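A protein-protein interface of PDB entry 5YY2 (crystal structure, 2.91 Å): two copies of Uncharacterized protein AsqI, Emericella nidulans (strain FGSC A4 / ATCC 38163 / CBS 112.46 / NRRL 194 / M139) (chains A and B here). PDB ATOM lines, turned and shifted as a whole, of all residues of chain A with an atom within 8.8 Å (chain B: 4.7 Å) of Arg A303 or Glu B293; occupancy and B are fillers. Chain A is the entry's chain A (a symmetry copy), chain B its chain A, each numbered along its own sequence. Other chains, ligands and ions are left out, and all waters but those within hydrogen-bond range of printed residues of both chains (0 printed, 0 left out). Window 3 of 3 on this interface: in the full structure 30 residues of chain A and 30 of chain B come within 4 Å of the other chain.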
ATOM      1  N   ASP A 296       9.131  19.655  24.085  1.00  0.00           N
ATOM      2  CA  ASP A 296       7.858  19.806  24.763  1.00  0.00           C
ATOM      3  C   ASP A 296       7.650  21.215  25.243  1.00  0.00           C
ATOM      4  O   ASP A 296       6.536  21.596  25.572  1.00  0.00           O
ATOM      5  CB  ASP A 296       7.783  18.870  25.954  1.00  0.00           C
ATOM      6  CG  ASP A 296       7.752  17.434  25.561  1.00  0.00           C
ATOM      7  OD1 ASP A 296       7.040  17.104  24.608  1.00  0.00           O
ATOM      8  OD2 ASP A 296       8.425  16.629  26.214  1.00  0.00           O
ATOM      9  N   ASN A 297       8.733  21.974  25.325  1.00  0.00           N
ATOM     10  CA  ASN A 297       8.668  23.316  25.865  1.00  0.00           C
ATOM     11  C   ASN A 297       8.347  24.311  24.792  1.00  0.00           C
ATOM     12  O   ASN A 297       7.638  25.278  25.018  1.00  0.00           O
ATOM     13  CB  ASN A 297       9.982  23.689  26.525  1.00  0.00           C
ATOM     14  CG  ASN A 297       9.991  23.385  27.976  1.00  0.00           C
ATOM     15  OD1 ASN A 297       8.955  23.072  28.549  1.00  0.00           O
ATOM     16  ND2 ASN A 297      11.156  23.486  28.597  1.00  0.00           N
ATOM     17  N   ILE A 298       8.912  24.066  23.622  1.00  0.00           N
ATOM     18  CA  ILE A 298       8.601  24.829  22.443  1.00  0.00           C
ATOM     19  C   ILE A 298       7.210  24.488  21.976  1.00  0.00           C
ATOM     20  O   ILE A 298       6.493  25.356  21.529  1.00  0.00           O
ATOM     21  CB  ILE A 298       9.584  24.564  21.327  1.00  0.00           C
ATOM     22  CG1 ILE A 298      10.983  24.964  21.764  1.00  0.00           C
ATOM     23  CG2 ILE A 298       9.204  25.353  20.099  1.00  0.00           C
ATOM     24  CD1 ILE A 298      11.961  25.006  20.658  1.00  0.00           C
ATOM     25  N   TYR A 299       6.816  23.224  22.083  1.00  0.00           N
ATOM     26  CA  TYR A 299       5.475  22.844  21.677  1.00  0.00           C
ATOM     27  C   TYR A 299       4.466  23.669  22.449  1.00  0.00           C
ATOM     28  O   TYR A 299       3.520  24.225  21.891  1.00  0.00           O
ATOM     29  CB  TYR A 299       5.177  21.374  21.944  1.00  0.00           C
ATOM     30  CG  TYR A 299       5.681  20.338  20.963  1.00  0.00           C
ATOM     31  CD1 TYR A 299       6.197  20.673  19.725  1.00  0.00           C
ATOM     32  CD2 TYR A 299       5.617  18.995  21.299  1.00  0.00           C
ATOM     33  CE1 TYR A 299       6.650  19.677  18.869  1.00  0.00           C
ATOM     34  CE2 TYR A 299       6.056  18.024  20.473  1.00  0.00           C
ATOM     35  CZ  TYR A 299       6.570  18.350  19.265  1.00  0.00           C
ATOM     36  OH  TYR A 299       6.997  17.314  18.480  1.00  0.00           O
ATOM     37  N   ALA A 300       4.685  23.734  23.751  1.00  0.00           N
ATOM     38  CA  ALA A 300       3.717  24.293  24.673  1.00  0.00           C
ATOM     39  C   ALA A 300       3.769  25.810  24.702  1.00  0.00           C
ATOM     40  O   ALA A 300       2.909  26.447  25.281  1.00  0.00           O
ATOM     41  CB  ALA A 300       3.937  23.723  26.063  1.00  0.00           C
ATOM     42  N   ALA A 301       4.781  26.386  24.076  1.00  0.00           N
ATOM     43  CA  ALA A 301       4.838  27.823  23.907  1.00  0.00           C
ATOM     44  C   ALA A 301       3.955  28.200  22.742  1.00  0.00           C
ATOM     45  O   ALA A 301       2.999  28.940  22.897  1.00  0.00           O
ATOM     46  CB  ALA A 301       6.252  28.286  23.670  1.00  0.00           C
ATOM     47  N   ILE A 302       4.278  27.656  21.575  1.00  0.00           N
ATOM     48  CA  ILE A 302       3.516  27.867  20.355  1.00  0.00           C
ATOM     49  C   ILE A 302       2.011  27.850  20.596  1.00  0.00           C
ATOM     50  O   ILE A 302       1.283  28.612  19.992  1.00  0.00           O
ATOM     51  CB  ILE A 302       3.866  26.801  19.301  1.00  0.00           C
ATOM     52  CG1 ILE A 302       5.329  26.908  18.897  1.00  0.00           C
ATOM     53  CG2 ILE A 302       2.994  26.955  18.076  1.00  0.00           C
ATOM     54  CD1 ILE A 302       5.720  25.977  17.804  1.00  0.00           C
ATOM     55  N   ARG A 303       1.548  27.004  21.504  1.00  0.00           N
ATOM     56  CA  ARG A 303       0.127  26.891  21.781  1.00  0.00           C
ATOM     57  C   ARG A 303      -0.341  28.017  22.679  1.00  0.00           C
ATOM     58  O   ARG A 303      -1.392  28.611  22.452  1.00  0.00           O
ATOM     59  CB  ARG A 303      -0.179  25.533  22.410  1.00  0.00           C
ATOM     60  CG  ARG A 303      -1.490  25.424  23.143  1.00  0.00           C
ATOM     61  CD  ARG A 303      -2.678  25.811  22.288  1.00  0.00           C
ATOM     62  NE  ARG A 303      -3.097  24.782  21.353  1.00  0.00           N
ATOM     63  CZ  ARG A 303      -3.931  25.012  20.346  1.00  0.00           C
ATOM     64  NH1 ARG A 303      -4.401  26.232  20.148  1.00  0.00           N
ATOM     65  NH2 ARG A 303      -4.280  24.035  19.533  1.00  0.00           N
ATOM     66  N   LYS A 304       0.440  28.331  23.700  1.00  0.00           N
ATOM     67  CA  LYS A 304       0.084  29.428  24.595  1.00  0.00           C
ATOM     68  C   LYS A 304       0.151  30.757  23.857  1.00  0.00           C
ATOM     69  O   LYS A 304      -0.601  31.675  24.145  1.00  0.00           O
ATOM     70  CB  LYS A 304       0.996  29.450  25.814  1.00  0.00           C
ATOM     71  CG  LYS A 304       0.734  30.595  26.740  1.00  0.00           C
ATOM     72  CD  LYS A 304       0.401  30.122  28.127  1.00  0.00           C
ATOM     73  CE  LYS A 304       1.586  30.273  29.049  1.00  0.00           C
ATOM     74  NZ  LYS A 304       1.363  29.553  30.329  1.00  0.00           N
ATOM     75  N   GLY A 305       1.060  30.846  22.902  1.00  0.00           N
ATOM     76  CA  GLY A 305       1.159  32.007  22.052  1.00  0.00           C
ATOM     77  C   GLY A 305       2.366  32.838  22.382  1.00  0.00           C
ATOM     78  O   GLY A 305       2.616  33.838  21.740  1.00  0.00           O
ATOM     79  N   GLN A 306       3.118  32.430  23.394  1.00  0.00           N
ATOM     80  CA  GLN A 306       4.234  33.243  23.871  1.00  0.00           C
ATOM     81  C   GLN A 306       5.498  32.461  24.154  1.00  0.00           C
ATOM     82  O   GLN A 306       5.443  31.296  24.500  1.00  0.00           O
ATOM     83  CB  GLN A 306       3.859  33.972  25.153  1.00  0.00           C
ATOM     84  CG  GLN A 306       2.403  34.350  25.300  1.00  0.00           C
ATOM     85  CD  GLN A 306       2.013  34.465  26.747  1.00  0.00           C
ATOM     86  OE1 GLN A 306       2.838  34.260  27.636  1.00  0.00           O
ATOM     87  NE2 GLN A 306       0.756  34.787  26.997  1.00  0.00           N
ATOM     88  N   PHE A 307       6.640  33.118  24.040  1.00  0.00           N
ATOM     89  CA  PHE A 307       7.883  32.523  24.499  1.00  0.00           C
ATOM     90  C   PHE A 307       8.334  33.212  25.770  1.00  0.00           C
ATOM     91  O   PHE A 307       8.510  34.414  25.777  1.00  0.00           O
ATOM     92  CB  PHE A 307       8.968  32.607  23.431  1.00  0.00           C
ATOM     93  CG  PHE A 307       8.937  31.474  22.461  1.00  0.00           C
ATOM     94  CD1 PHE A 307       9.313  30.213  22.850  1.00  0.00           C
ATOM     95  CD2 PHE A 307       8.523  31.664  21.171  1.00  0.00           C
ATOM     96  CE1 PHE A 307       9.278  29.163  21.975  1.00  0.00           C
ATOM     97  CE2 PHE A 307       8.485  30.615  20.293  1.00  0.00           C
ATOM     98  CZ  PHE A 307       8.869  29.361  20.700  1.00  0.00           C
ATOM     99  N   LEU A 318       3.688  35.767  20.386  1.00  0.00           N
ATOM    100  CA  LEU A 318       3.710  35.421  18.985  1.00  0.00           C
ATOM    101  C   LEU A 318       2.596  36.157  18.289  1.00  0.00           C
ATOM    102  O   LEU A 318       1.453  36.140  18.733  1.00  0.00           O
ATOM    103  CB  LEU A 318       3.563  33.916  18.787  1.00  0.00           C
ATOM    104  CG  LEU A 318       4.721  33.087  19.326  1.00  0.00           C
ATOM    105  CD1 LEU A 318       4.347  31.639  19.292  1.00  0.00           C
ATOM    106  CD2 LEU A 318       5.937  33.342  18.494  1.00  0.00           C
ATOM    107  N   VAL A 327       9.809  30.864  16.233  1.00  0.00           N
ATOM    108  CA  VAL A 327       9.814  29.411  16.303  1.00  0.00           C
ATOM    109  C   VAL A 327      11.015  28.851  15.554  1.00  0.00           C
ATOM    110  O   VAL A 327      11.775  28.070  16.092  1.00  0.00           O
ATOM    111  CB  VAL A 327       8.540  28.812  15.730  1.00  0.00           C
ATOM    112  CG1 VAL A 327       8.722  27.341  15.482  1.00  0.00           C
ATOM    113  CG2 VAL A 327       7.399  29.045  16.680  1.00  0.00           C
ATOM    114  N   LEU A 406       2.389  23.530  13.250  1.00  0.00           N
ATOM    115  CA  LEU A 406       1.733  23.925  14.478  1.00  0.00           C
ATOM    116  C   LEU A 406       1.466  25.404  14.497  1.00  0.00           C
ATOM    117  O   LEU A 406       0.403  25.838  14.871  1.00  0.00           O
ATOM    118  CB  LEU A 406       2.583  23.550  15.677  1.00  0.00           C
ATOM    119  CG  LEU A 406       2.597  22.080  16.021  1.00  0.00           C
ATOM    120  CD1 LEU A 406       3.556  21.844  17.152  1.00  0.00           C
ATOM    121  CD2 LEU A 406       1.209  21.633  16.384  1.00  0.00           C
ATOM    122  N   ALA A 407       2.458  26.175  14.094  1.00  0.00           N
ATOM    123  CA  ALA A 407       2.372  27.613  14.181  1.00  0.00           C
ATOM    124  C   ALA A 407       1.529  28.170  13.056  1.00  0.00           C
ATOM    125  O   ALA A 407       0.837  29.161  13.223  1.00  0.00           O
ATOM    126  CB  ALA A 407       3.739  28.216  14.153  1.00  0.00           C
ATOM    127  N   THR A 409      -1.211  27.074  11.617  1.00  0.00           N
ATOM    128  CA  THR A 409      -2.663  27.081  11.780  1.00  0.00           C
ATOM    129  C   THR A 409      -3.124  27.842  13.014  1.00  0.00           C
ATOM    130  O   THR A 409      -4.315  28.041  13.206  1.00  0.00           O
ATOM    131  CB  THR A 409      -3.247  25.670  11.848  1.00  0.00           C
ATOM    132  OG1 THR A 409      -2.639  24.964  12.917  1.00  0.00           O
ATOM    133  CG2 THR A 409      -2.996  24.925  10.562  1.00  0.00           C
ATOM    134  N   ARG A 410      -2.183  28.270  13.844  1.00  0.00           N
ATOM    135  CA  ARG A 410      -2.495  29.097  14.998  1.00  0.00           C
ATOM    136  C   ARG A 410      -2.669  30.558  14.602  1.00  0.00           C
ATOM    137  O   ARG A 410      -3.408  31.299  15.237  1.00  0.00           O
ATOM    138  CB  ARG A 410      -1.401  28.967  16.047  1.00  0.00           C
ATOM    139  CG  ARG A 410      -1.463  27.674  16.821  1.00  0.00           C
ATOM    140  CD  ARG A 410      -2.277  27.807  18.091  1.00  0.00           C
ATOM    141  NE  ARG A 410      -1.720  28.862  18.905  1.00  0.00           N
ATOM    142  CZ  ARG A 410      -2.430  29.848  19.433  1.00  0.00           C
ATOM    143  NH1 ARG A 410      -3.742  29.909  19.247  1.00  0.00           N
ATOM    144  NH2 ARG A 410      -1.824  30.772  20.159  1.00  0.00           N
ATOM    145  N   TYR A 411      -1.994  30.950  13.532  1.00  0.00           N
ATOM    146  CA  TYR A 411      -1.964  32.325  13.061  1.00  0.00           C
ATOM    147  C   TYR A 411      -2.267  32.423  11.574  1.00  0.00           C
ATOM    148  O   TYR A 411      -1.394  32.658  10.772  1.00  0.00           O
ATOM    149  CB  TYR A 411      -0.600  32.937  13.359  1.00  0.00           C
ATOM    150  CG  TYR A 411      -0.317  32.955  14.829  1.00  0.00           C
ATOM    151  CD1 TYR A 411      -0.758  34.001  15.614  1.00  0.00           C
ATOM    152  CD2 TYR A 411       0.349  31.907  15.447  1.00  0.00           C
ATOM    153  CE1 TYR A 411      -0.531  34.016  16.972  1.00  0.00           C
ATOM    154  CE2 TYR A 411       0.580  31.916  16.803  1.00  0.00           C
ATOM    155  CZ  TYR A 411       0.135  32.975  17.562  1.00  0.00           C
ATOM    156  OH  TYR A 411       0.349  33.012  18.919  1.00  0.00           O
ATOM    157  N   ALA B 289      -9.111  21.907  14.822  1.00  0.00           N
ATOM    158  CA  ALA B 289      -8.269  22.700  15.702  1.00  0.00           C
ATOM    159  C   ALA B 289      -8.672  22.539  17.147  1.00  0.00           C
ATOM    160  O   ALA B 289      -7.920  22.898  18.038  1.00  0.00           O
ATOM    161  CB  ALA B 289      -8.320  24.155  15.304  1.00  0.00           C
ATOM    162  N   ARG B 290      -9.865  22.011  17.391  1.00  0.00           N
ATOM    163  CA  ARG B 290     -10.305  21.839  18.763  1.00  0.00           C
ATOM    164  C   ARG B 290      -9.625  20.614  19.351  1.00  0.00           C
ATOM    165  O   ARG B 290      -9.046  20.675  20.419  1.00  0.00           O
ATOM    166  CB  ARG B 290     -11.821  21.712  18.871  1.00  0.00           C
ATOM    167  CG  ARG B 290     -12.276  21.869  20.309  1.00  0.00           C
ATOM    168  CD  ARG B 290     -13.776  21.880  20.494  1.00  0.00           C
ATOM    169  NE  ARG B 290     -14.097  22.199  21.884  1.00  0.00           N
ATOM    170  CZ  ARG B 290     -15.290  22.024  22.448  1.00  0.00           C
ATOM    171  NH1 ARG B 290     -16.299  21.526  21.750  1.00  0.00           N
ATOM    172  NH2 ARG B 290     -15.472  22.339  23.720  1.00  0.00           N
ATOM    173  N   LEU B 291      -9.689  19.500  18.634  1.00  0.00           N
ATOM    174  CA  LEU B 291      -8.964  18.304  19.008  1.00  0.00           C
ATOM    175  C   LEU B 291      -7.498  18.602  19.189  1.00  0.00           C
ATOM    176  O   LEU B 291      -6.883  18.144  20.124  1.00  0.00           O
ATOM    177  CB  LEU B 291      -9.138  17.225  17.958  1.00  0.00           C
ATOM    178  CG  LEU B 291     -10.546  16.688  17.787  1.00  0.00           C
ATOM    179  CD1 LEU B 291     -10.666  16.230  16.403  1.00  0.00           C
ATOM    180  CD2 LEU B 291     -10.807  15.531  18.705  1.00  0.00           C
ATOM    181  N   GLU B 292      -6.935  19.385  18.291  1.00  0.00           N
ATOM    182  CA  GLU B 292      -5.525  19.725  18.385  1.00  0.00           C
ATOM    183  C   GLU B 292      -5.230  20.479  19.664  1.00  0.00           C
ATOM    184  O   GLU B 292      -4.116  20.456  20.173  1.00  0.00           O
ATOM    185  CB  GLU B 292      -5.086  20.561  17.189  1.00  0.00           C
ATOM    186  CG  GLU B 292      -5.175  19.858  15.862  1.00  0.00           C
ATOM    187  CD  GLU B 292      -4.403  20.583  14.814  1.00  0.00           C
ATOM    188  OE1 GLU B 292      -3.978  21.706  15.109  1.00  0.00           O
ATOM    189  OE2 GLU B 292      -4.209  20.037  13.717  1.00  0.00           O
ATOM    190  N   GLU B 293      -6.233  21.152  20.193  1.00  0.00           N
ATOM    191  CA  GLU B 293      -6.017  21.930  21.391  1.00  0.00           C
ATOM    192  C   GLU B 293      -5.924  21.019  22.579  1.00  0.00           C
ATOM    193  O   GLU B 293      -5.017  21.146  23.381  1.00  0.00           O
ATOM    194  CB  GLU B 293      -7.129  22.936  21.596  1.00  0.00           C
ATOM    195  CG  GLU B 293      -6.994  23.682  22.891  1.00  0.00           C
ATOM    196  CD  GLU B 293      -7.917  24.853  22.956  1.00  0.00           C
ATOM    197  OE1 GLU B 293      -7.434  25.948  23.294  1.00  0.00           O
ATOM    198  OE2 GLU B 293      -9.113  24.677  22.656  1.00  0.00           O
ATOM    199  N   TRP B 294      -6.879  20.104  22.687  1.00  0.00           N
ATOM    200  CA  TRP B 294      -6.852  19.070  23.709  1.00  0.00           C
ATOM    201  C   TRP B 294      -5.525  18.348  23.697  1.00  0.00           C
ATOM    202  O   TRP B 294      -4.869  18.223  24.719  1.00  0.00           O
ATOM    203  CB  TRP B 294      -7.979  18.070  23.496  1.00  0.00           C
ATOM    204  CG  TRP B 294      -9.313  18.690  23.597  1.00  0.00           C
ATOM    205  CD1 TRP B 294      -9.610  19.867  24.194  1.00  0.00           C
ATOM    206  CD2 TRP B 294     -10.538  18.193  23.060  1.00  0.00           C
ATOM    207  NE1 TRP B 294     -10.939  20.135  24.075  1.00  0.00           N
ATOM    208  CE2 TRP B 294     -11.534  19.119  23.382  1.00  0.00           C
ATOM    209  CE3 TRP B 294     -10.887  17.056  22.330  1.00  0.00           C
ATOM    210  CZ2 TRP B 294     -12.855  18.945  23.013  1.00  0.00           C
ATOM    211  CZ3 TRP B 294     -12.200  16.885  21.966  1.00  0.00           C
ATOM    212  CH2 TRP B 294     -13.167  17.822  22.304  1.00  0.00           C
ATOM    213  N   ARG B 295      -5.130  17.883  22.523  1.00  0.00           N
ATOM    214  CA  ARG B 295      -3.873  17.173  22.376  1.00  0.00           C
ATOM    215  C   ARG B 295      -2.739  17.963  23.009  1.00  0.00           C
ATOM    216  O   ARG B 295      -2.061  17.487  23.906  1.00  0.00           O
ATOM    217  CB  ARG B 295      -3.570  16.915  20.904  1.00  0.00           C
ATOM    218  CG  ARG B 295      -2.201  16.329  20.645  1.00  0.00           C
ATOM    219  CD  ARG B 295      -1.850  16.426  19.167  1.00  0.00           C
ATOM    220  NE  ARG B 295      -1.459  17.779  18.802  1.00  0.00           N
ATOM    221  CZ  ARG B 295      -1.446  18.251  17.564  1.00  0.00           C
ATOM    222  NH1 ARG B 295      -1.820  17.492  16.554  1.00  0.00           N
ATOM    223  NH2 ARG B 295      -1.069  19.492  17.338  1.00  0.00           N
ATOM    224  N   ASP B 296      -2.569  19.197  22.555  1.00  0.00           N
ATOM    225  CA  ASP B 296      -1.482  20.048  23.001  1.00  0.00           C
ATOM    226  C   ASP B 296      -1.595  20.367  24.465  1.00  0.00           C
ATOM    227  O   ASP B 296      -0.637  20.821  25.074  1.00  0.00           O
ATOM    228  CB  ASP B 296      -1.474  21.346  22.218  1.00  0.00           C
ATOM    229  CG  ASP B 296      -1.140  21.153  20.781  1.00  0.00           C
ATOM    230  OD1 ASP B 296      -0.223  20.379  20.492  1.00  0.00           O
ATOM    231  OD2 ASP B 296      -1.781  21.788  19.935  1.00  0.00           O
ATOM    232  N   ASN B 297      -2.784  20.174  25.019  1.00  0.00           N
ATOM    233  CA  ASN B 297      -3.037  20.538  26.398  1.00  0.00           C
ATOM    234  C   ASN B 297      -2.691  19.411  27.323  1.00  0.00           C
ATOM    235  O   ASN B 297      -2.201  19.621  28.420  1.00  0.00           O
ATOM    236  CB  ASN B 297      -4.492  20.922  26.589  1.00  0.00           C
ATOM    237  CG  ASN B 297      -4.715  22.379  26.435  1.00  0.00           C
ATOM    238  OD1 ASN B 297      -3.765  23.149  26.375  1.00  0.00           O
ATOM    239  ND2 ASN B 297      -5.975  22.786  26.383  1.00  0.00           N
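NH2 of Arg A303 is in salt-bridge range of OD2 of Asp B296.
The side-chain carboxylate (OD1) of Asp B296 lies within salt-bridge range of the guanidinium group (NE) of Arg B295, 3.3 Å away.
The backbone carbonyl oxygen (O) of Glu B292 lies close to the side-chain carboxylate (OD2) of Asp B296, at 2.7 Å.
O of Arg A303 sits at hydrogen-bond distance from NH2 of Arg A410, at 3.2 Å.
O of Glu B292 touches NH2 of Arg A303 (3.6 Å).
NH2 of Arg A303 touches CA of Glu B293, at 3.3 Å.
CD2 of Leu A406 touches NH2 of Arg B295 (3.3 Å).
Arg A303 touches three residues of chain B.
Of the printed residues of chain A, Arg B295 touches Leu A406 (3.3 Å).
Of the printed residues of chain B, Leu A406 touches Arg B295.
Of the printed residues of chain A, Glu B292 touches Arg A303 (3.6 Å).
Leu A318 touches none of the printed residues of chain B.
Val A327 touches none of the printed residues of chain B.
The nearest residue of chain A that does not touch Glu B293 is Arg A410 (6.8 Å).
The nearest printed residue of chain A that does not touch Glu B292 is Thr A409 (4.1 Å).
Of the 19 printed residues of chain A, 2 touch a printed residue of chain B.
Positions printed for both chains: 296 and 297.
Of the 4 pairs that touch across the chains among the printed residues, none has its exchanged pair printed and touching as well.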
